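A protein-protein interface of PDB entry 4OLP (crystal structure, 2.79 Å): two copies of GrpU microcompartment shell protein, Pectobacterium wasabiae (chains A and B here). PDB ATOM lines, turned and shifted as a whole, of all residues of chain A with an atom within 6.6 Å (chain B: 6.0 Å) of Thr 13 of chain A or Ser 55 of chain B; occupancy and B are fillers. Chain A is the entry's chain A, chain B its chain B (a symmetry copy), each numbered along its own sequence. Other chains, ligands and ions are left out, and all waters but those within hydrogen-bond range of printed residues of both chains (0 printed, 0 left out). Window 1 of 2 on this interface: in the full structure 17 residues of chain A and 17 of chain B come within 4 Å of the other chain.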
ATOM      1  N   ILE A   6      25.672  32.564  16.837  1.00  0.00           N
ATOM      2  CA  ILE A   6      25.513  32.569  15.400  1.00  0.00           C
ATOM      3  C   ILE A   6      25.670  33.995  14.941  1.00  0.00           C
ATOM      4  O   ILE A   6      24.860  34.855  15.257  1.00  0.00           O
ATOM      5  CB  ILE A   6      24.129  32.042  14.995  1.00  0.00           C
ATOM      6  CG1 ILE A   6      24.019  30.566  15.387  1.00  0.00           C
ATOM      7  CG2 ILE A   6      23.891  32.217  13.494  1.00  0.00           C
ATOM      8  CD1 ILE A   6      22.600  30.059  15.488  1.00  0.00           C
ATOM      9  N   PRO A   9      22.948  35.666  11.080  1.00  0.00           N
ATOM     10  CA  PRO A   9      22.151  34.491  10.778  1.00  0.00           C
ATOM     11  C   PRO A   9      21.365  34.651   9.492  1.00  0.00           C
ATOM     12  O   PRO A   9      20.970  35.755   9.152  1.00  0.00           O
ATOM     13  CB  PRO A   9      21.200  34.396  11.974  1.00  0.00           C
ATOM     14  CG  PRO A   9      21.105  35.796  12.490  1.00  0.00           C
ATOM     15  CD  PRO A   9      22.491  36.339  12.311  1.00  0.00           C
ATOM     16  N   THR A  10      21.129  33.531   8.817  1.00  0.00           N
ATOM     17  CA  THR A  10      20.299  33.488   7.603  1.00  0.00           C
ATOM     18  C   THR A  10      18.852  33.771   7.965  1.00  0.00           C
ATOM     19  O   THR A  10      18.481  33.747   9.137  1.00  0.00           O
ATOM     20  CB  THR A  10      20.341  32.120   6.882  1.00  0.00           C
ATOM     21  OG1 THR A  10      19.872  31.082   7.751  1.00  0.00           O
ATOM     22  CG2 THR A  10      21.739  31.821   6.425  1.00  0.00           C
ATOM     23  N   LEU A  11      18.039  34.026   6.952  1.00  0.00           N
ATOM     24  CA  LEU A  11      16.595  34.145   7.138  1.00  0.00           C
ATOM     25  C   LEU A  11      15.992  32.798   7.550  1.00  0.00           C
ATOM     26  O   LEU A  11      15.155  32.742   8.445  1.00  0.00           O
ATOM     27  CB  LEU A  11      15.922  34.651   5.853  1.00  0.00           C
ATOM     28  CG  LEU A  11      16.261  36.079   5.396  1.00  0.00           C
ATOM     29  CD1 LEU A  11      15.759  36.322   3.980  1.00  0.00           C
ATOM     30  CD2 LEU A  11      15.696  37.119   6.351  1.00  0.00           C
ATOM     31  N   GLU A  12      16.418  31.739   6.867  1.00  0.00           N
ATOM     32  CA  GLU A  12      16.106  30.344   7.196  1.00  0.00           C
ATOM     33  C   GLU A  12      16.472  29.954   8.654  1.00  0.00           C
ATOM     34  O   GLU A  12      15.713  29.252   9.352  1.00  0.00           O
ATOM     35  CB  GLU A  12      16.901  29.478   6.195  1.00  0.00           C
ATOM     36  CG  GLU A  12      16.236  28.229   5.662  1.00  0.00           C
ATOM     37  CD  GLU A  12      17.107  27.598   4.582  1.00  0.00           C
ATOM     38  OE1 GLU A  12      18.299  27.440   4.870  1.00  0.00           O
ATOM     39  OE2 GLU A  12      16.647  27.292   3.453  1.00  0.00           O
ATOM     40  N   THR A  13      17.602  30.451   9.143  1.00  0.00           N
ATOM     41  CA  THR A  13      17.957  30.227  10.534  1.00  0.00           C
ATOM     42  C   THR A  13      16.949  30.908  11.471  1.00  0.00           C
ATOM     43  O   THR A  13      16.487  30.317  12.465  1.00  0.00           O
ATOM     44  CB  THR A  13      19.371  30.740  10.827  1.00  0.00           C
ATOM     45  OG1 THR A  13      20.313  30.000  10.038  1.00  0.00           O
ATOM     46  CG2 THR A  13      19.705  30.561  12.299  1.00  0.00           C
ATOM     47  N   LEU A  14      16.610  32.155  11.156  1.00  0.00           N
ATOM     48  CA  LEU A  14      15.607  32.889  11.929  1.00  0.00           C
ATOM     49  C   LEU A  14      14.267  32.169  11.889  1.00  0.00           C
ATOM     50  O   LEU A  14      13.590  32.061  12.900  1.00  0.00           O
ATOM     51  CB  LEU A  14      15.453  34.294  11.390  1.00  0.00           C
ATOM     52  CG  LEU A  14      16.688  35.162  11.606  1.00  0.00           C
ATOM     53  CD1 LEU A  14      16.687  36.342  10.645  1.00  0.00           C
ATOM     54  CD2 LEU A  14      16.737  35.629  13.045  1.00  0.00           C
ATOM     55  N   ALA A  15      13.892  31.670  10.717  1.00  0.00           N
ATOM     56  CA  ALA A  15      12.632  30.940  10.549  1.00  0.00           C
ATOM     57  C   ALA A  15      12.570  29.688  11.420  1.00  0.00           C
ATOM     58  O   ALA A  15      11.536  29.386  12.005  1.00  0.00           O
ATOM     59  CB  ALA A  15      12.427  30.580   9.084  1.00  0.00           C
ATOM     60  N   MET A  16      13.692  28.980  11.524  1.00  0.00           N
ATOM     61  CA  MET A  16      13.768  27.762  12.337  1.00  0.00           C
ATOM     62  C   MET A  16      13.585  28.080  13.815  1.00  0.00           C
ATOM     63  O   MET A  16      12.881  27.359  14.538  1.00  0.00           O
ATOM     64  CB  MET A  16      15.105  27.048  12.110  1.00  0.00           C
ATOM     65  CG  MET A  16      15.079  26.167  10.875  1.00  0.00           C
ATOM     66  SD  MET A  16      16.661  25.555  10.303  1.00  0.00           S
ATOM     67  CE  MET A  16      17.149  24.431  11.610  1.00  0.00           C
ATOM     68  N   LEU A  17      14.218  29.165  14.254  1.00  0.00           N
ATOM     69  CA  LEU A  17      14.123  29.589  15.640  1.00  0.00           C
ATOM     70  C   LEU A  17      12.743  30.084  15.983  1.00  0.00           C
ATOM     71  O   LEU A  17      12.226  29.744  17.055  1.00  0.00           O
ATOM     72  CB  LEU A  17      15.165  30.662  15.971  1.00  0.00           C
ATOM     73  CG  LEU A  17      16.583  30.092  15.989  1.00  0.00           C
ATOM     74  CD1 LEU A  17      17.587  31.221  16.067  1.00  0.00           C
ATOM     75  CD2 LEU A  17      16.807  29.130  17.146  1.00  0.00           C
ATOM     76  N   LYS A  18      12.145  30.866  15.081  1.00  0.00           N
ATOM     77  CA  LYS A  18      10.792  31.410  15.283  1.00  0.00           C
ATOM     78  C   LYS A  18       9.757  30.323  15.469  1.00  0.00           C
ATOM     79  O   LYS A  18       8.877  30.449  16.313  1.00  0.00           O
ATOM     80  CB  LYS A  18      10.386  32.343  14.140  1.00  0.00           C
ATOM     81  CG  LYS A  18      11.073  33.690  14.247  1.00  0.00           C
ATOM     82  CD  LYS A  18      10.551  34.720  13.275  1.00  0.00           C
ATOM     83  CE  LYS A  18      11.070  36.095  13.662  1.00  0.00           C
ATOM     84  NZ  LYS A  18      10.465  37.169  12.835  1.00  0.00           N
ATOM     85  N   ILE A  37      23.016  35.821  17.250  1.00  0.00           N
ATOM     86  CA  ILE A  37      22.157  35.077  18.161  1.00  0.00           C
ATOM     87  C   ILE A  37      23.009  34.190  19.071  1.00  0.00           C
ATOM     88  O   ILE A  37      23.794  33.360  18.604  1.00  0.00           O
ATOM     89  CB  ILE A  37      21.176  34.178  17.402  1.00  0.00           C
ATOM     90  CG1 ILE A  37      20.342  35.002  16.416  1.00  0.00           C
ATOM     91  CG2 ILE A  37      20.269  33.467  18.387  1.00  0.00           C
ATOM     92  CD1 ILE A  37      19.533  34.173  15.439  1.00  0.00           C
ATOM     93  N   TYR B  48      21.260  24.647  15.597  1.00  0.00           N
ATOM     94  CA  TYR B  48      21.038  25.871  14.856  1.00  0.00           C
ATOM     95  C   TYR B  48      22.335  26.514  14.419  1.00  0.00           C
ATOM     96  O   TYR B  48      22.377  27.157  13.368  1.00  0.00           O
ATOM     97  CB  TYR B  48      20.234  26.848  15.682  1.00  0.00           C
ATOM     98  CG  TYR B  48      18.863  26.327  15.925  1.00  0.00           C
ATOM     99  CD1 TYR B  48      18.019  26.069  14.865  1.00  0.00           C
ATOM    100  CD2 TYR B  48      18.412  26.064  17.205  1.00  0.00           C
ATOM    101  CE1 TYR B  48      16.749  25.585  15.066  1.00  0.00           C
ATOM    102  CE2 TYR B  48      17.141  25.573  17.421  1.00  0.00           C
ATOM    103  CZ  TYR B  48      16.316  25.343  16.343  1.00  0.00           C
ATOM    104  OH  TYR B  48      15.047  24.869  16.519  1.00  0.00           O
ATOM    105  N   TYR B  50      25.113  24.846  13.510  1.00  0.00           N
ATOM    106  CA  TYR B  50      25.548  24.108  12.346  1.00  0.00           C
ATOM    107  C   TYR B  50      24.569  24.183  11.175  1.00  0.00           C
ATOM    108  O   TYR B  50      25.009  24.148  10.035  1.00  0.00           O
ATOM    109  CB  TYR B  50      25.908  22.667  12.728  1.00  0.00           C
ATOM    110  CG  TYR B  50      27.223  22.587  13.482  1.00  0.00           C
ATOM    111  CD1 TYR B  50      28.411  22.986  12.882  1.00  0.00           C
ATOM    112  CD2 TYR B  50      27.264  22.133  14.799  1.00  0.00           C
ATOM    113  CE1 TYR B  50      29.604  22.925  13.584  1.00  0.00           C
ATOM    114  CE2 TYR B  50      28.448  22.072  15.504  1.00  0.00           C
ATOM    115  CZ  TYR B  50      29.620  22.468  14.897  1.00  0.00           C
ATOM    116  OH  TYR B  50      30.807  22.390  15.610  1.00  0.00           O
ATOM    117  N   ALA B  51      23.268  24.324  11.442  1.00  0.00           N
ATOM    118  CA  ALA B  51      22.278  24.521  10.362  1.00  0.00           C
ATOM    119  C   ALA B  51      22.550  25.803   9.605  1.00  0.00           C
ATOM    120  O   ALA B  51      22.592  25.854   8.378  1.00  0.00           O
ATOM    121  CB  ALA B  51      20.874  24.579  10.915  1.00  0.00           C
ATOM    122  N   ASP B  52      22.797  26.843  10.378  1.00  0.00           N
ATOM    123  CA  ASP B  52      23.022  28.153   9.841  1.00  0.00           C
ATOM    124  C   ASP B  52      24.241  28.107   8.908  1.00  0.00           C
ATOM    125  O   ASP B  52      24.210  28.663   7.805  1.00  0.00           O
ATOM    126  CB  ASP B  52      23.242  29.121  10.996  1.00  0.00           C
ATOM    127  CG  ASP B  52      23.671  30.484  10.530  1.00  0.00           C
ATOM    128  OD1 ASP B  52      22.796  31.233  10.060  1.00  0.00           O
ATOM    129  OD2 ASP B  52      24.887  30.794  10.640  1.00  0.00           O
ATOM    130  N   GLN B  53      25.299  27.439   9.370  1.00  0.00           N
ATOM    131  CA  GLN B  53      26.493  27.198   8.572  1.00  0.00           C
ATOM    132  C   GLN B  53      26.087  26.596   7.233  1.00  0.00           C
ATOM    133  O   GLN B  53      26.345  27.149   6.154  1.00  0.00           O
ATOM    134  CB  GLN B  53      27.378  26.145   9.330  1.00  0.00           C
ATOM    135  CG  GLN B  53      28.122  26.572  10.590  1.00  0.00           C
ATOM    136  CD  GLN B  53      29.190  27.570  10.276  1.00  0.00           C
ATOM    137  OE1 GLN B  53      28.903  28.634   9.733  1.00  0.00           O
ATOM    138  NE2 GLN B  53      30.441  27.230  10.593  1.00  0.00           N
ATOM    139  N   ALA B  54      25.396  25.472   7.322  1.00  0.00           N
ATOM    140  CA  ALA B  54      24.959  24.732   6.153  1.00  0.00           C
ATOM    141  C   ALA B  54      24.051  25.532   5.240  1.00  0.00           C
ATOM    142  O   ALA B  54      24.103  25.377   4.013  1.00  0.00           O
ATOM    143  CB  ALA B  54      24.227  23.485   6.582  1.00  0.00           C
ATOM    144  N   SER B  55      23.197  26.363   5.829  1.00  0.00           N
ATOM    145  CA  SER B  55      22.299  27.169   5.023  1.00  0.00           C
ATOM    146  C   SER B  55      23.095  28.202   4.234  1.00  0.00           C
ATOM    147  O   SER B  55      22.694  28.577   3.130  1.00  0.00           O
ATOM    148  CB  SER B  55      21.255  27.841   5.896  1.00  0.00           C
ATOM    149  OG  SER B  55      21.828  28.898   6.623  1.00  0.00           O
ATOM    150  N   LYS B  56      24.224  28.639   4.788  1.00  0.00           N
ATOM    151  CA  LYS B  56      25.094  29.591   4.098  1.00  0.00           C
ATOM    152  C   LYS B  56      25.893  28.880   3.015  1.00  0.00           C
ATOM    153  O   LYS B  56      26.308  29.502   2.043  1.00  0.00           O
ATOM    154  CB  LYS B  56      26.032  30.307   5.076  1.00  0.00           C
ATOM    155  CG  LYS B  56      25.301  31.258   5.983  1.00  0.00           C
ATOM    156  CD  LYS B  56      26.149  31.692   7.160  1.00  0.00           C
ATOM    157  CE  LYS B  56      25.475  32.825   7.926  1.00  0.00           C
ATOM    158  NZ  LYS B  56      26.010  32.968   9.308  1.00  0.00           N
ATOM    159  N   SER B  57      26.117  27.583   3.197  1.00  0.00           N
ATOM    160  CA  SER B  57      26.862  26.806   2.219  1.00  0.00           C
ATOM    161  C   SER B  57      25.996  26.429   1.026  1.00  0.00           C
ATOM    162  O   SER B  57      24.831  26.075   1.164  1.00  0.00           O
ATOM    163  CB  SER B  57      27.450  25.521   2.834  1.00  0.00           C
ATOM    164  OG  SER B  57      28.318  25.767   3.940  1.00  0.00           O
ATOM    165  N   ALA B  58      26.603  26.455  -0.154  1.00  0.00           N
ATOM    166  CA  ALA B  58      25.899  26.030  -1.348  1.00  0.00           C
ATOM    167  C   ALA B  58      25.910  24.520  -1.279  1.00  0.00           C
ATOM    168  O   ALA B  58      26.634  23.960  -0.464  1.00  0.00           O
ATOM    169  CB  ALA B  58      26.596  26.513  -2.604  1.00  0.00           C
ATOM    170  N   VAL B  60      24.250  22.272  -0.010  1.00  0.00           N
ATOM    171  CA  VAL B  60      23.528  21.540   1.007  1.00  0.00           C
ATOM    172  C   VAL B  60      22.322  22.345   1.465  1.00  0.00           C
ATOM    173  O   VAL B  60      22.237  23.555   1.406  1.00  0.00           O
ATOM    174  CB  VAL B  60      24.349  21.091   2.258  1.00  0.00           C
ATOM    175  CG1 VAL B  60      25.572  20.260   1.879  1.00  0.00           C
ATOM    176  CG2 VAL B  60      24.786  22.294   3.086  1.00  0.00           C
ATOM    177  N   VAL B  62      19.499  22.044   4.916  1.00  0.00           N
ATOM    178  CA  VAL B  62      19.423  21.519   6.273  1.00  0.00           C
ATOM    179  C   VAL B  62      18.010  21.558   6.786  1.00  0.00           C
ATOM    180  O   VAL B  62      17.193  22.401   6.378  1.00  0.00           O
ATOM    181  CB  VAL B  62      20.289  22.291   7.288  1.00  0.00           C
ATOM    182  CG1 VAL B  62      21.737  21.862   7.144  1.00  0.00           C
ATOM    183  CG2 VAL B  62      20.132  23.802   7.124  1.00  0.00           C
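No position is printed for both chains.
Thr 13 of chain A touches just these residues of chain B: Asp 52 (2.8 Å) and Ser 55 (3.9 Å). Printed residues of chain A within 4 Å of Ser 55 of chain B: Thr 10, Glu 12 and Thr 13. Of the printed residues of chain B, Leu 17 of chain A touches Tyr 48. Of the printed residues of chain A, Lys 56 of chain B touches Thr 10 (3.6 Å). The nearest residue of chain A that does not touch Ser 55 of chain B is Leu 11 of chain A (6.4 Å). The nearest printed residue of chain B that does not touch Glu 12 of chain A is Val 62 of chain B (4.7 Å).
OG of Ser 55 of chain B sits close to OG1 of Thr 10 of chain A (3.1 Å). OD1 of Asp 52 of chain B is in hydrogen-bond range of N of Thr 10 of chain A (3.1 Å). The side-chain carboxylate of Asp 52 of chain B is in hydrogen-bond range of the side-chain hydroxyl of Thr 13 of chain A (2.8 Å).
Among the printed residues, 12 pairs touch across the chains. Among the printed residues, no Asp or Glu carboxylate lies within 4 Å of a Lys or Arg side-chain nitrogen of the other chain.
Tyr 48 of chain B touches Ile 6 of chain A (O to CD1, 3.6 Å). OD2 of Asp 52 of chain B touches CG2 of Ile 6 of chain A, 3.3 Å away. Asp 52 of chain B touches Pro 9 of chain A. Thr 10 of chain A touches Lys 56 of chain B (CG2 to CG, 3.6 Å). Ser 55 of chain B touches Glu 12 of chain A (CB to OE1, 3.2 Å). Thr 13 of chain A touches Ser 55 of chain B. CE1 of Tyr 48 of chain B touches CE of Met 16 of chain A, at 3.7 Å. CE of Met 16 of chain A touches CB of Ala 51 of chain B, at 3.8 Å. Tyr 48 of chain B touches Leu 17 of chain A (CD2 to CD2, 3.5 Å).
The side-chain carboxylate of Asp 52 of chain B lies within salt-bridge range of the side-chain amino group of Lys 56 of chain B. The side-chain hydroxyl of Thr 10 of chain A sits at hydrogen-bond distance from the side-chain hydroxyl of Thr 13 of chain A, at 2.6 Å. The backbone NH (N) of Ile 6 of chain A is in hydrogen-bond range of the backbone carbonyl oxygen (O) of Ile 37 of chain A, 2.7 Å away. The backbone carbonyl oxygen (O) of Asp 52 of chain B is in hydrogen-bond range of the side-chain hydroxyl (OG) of Ser 55 of chain B.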
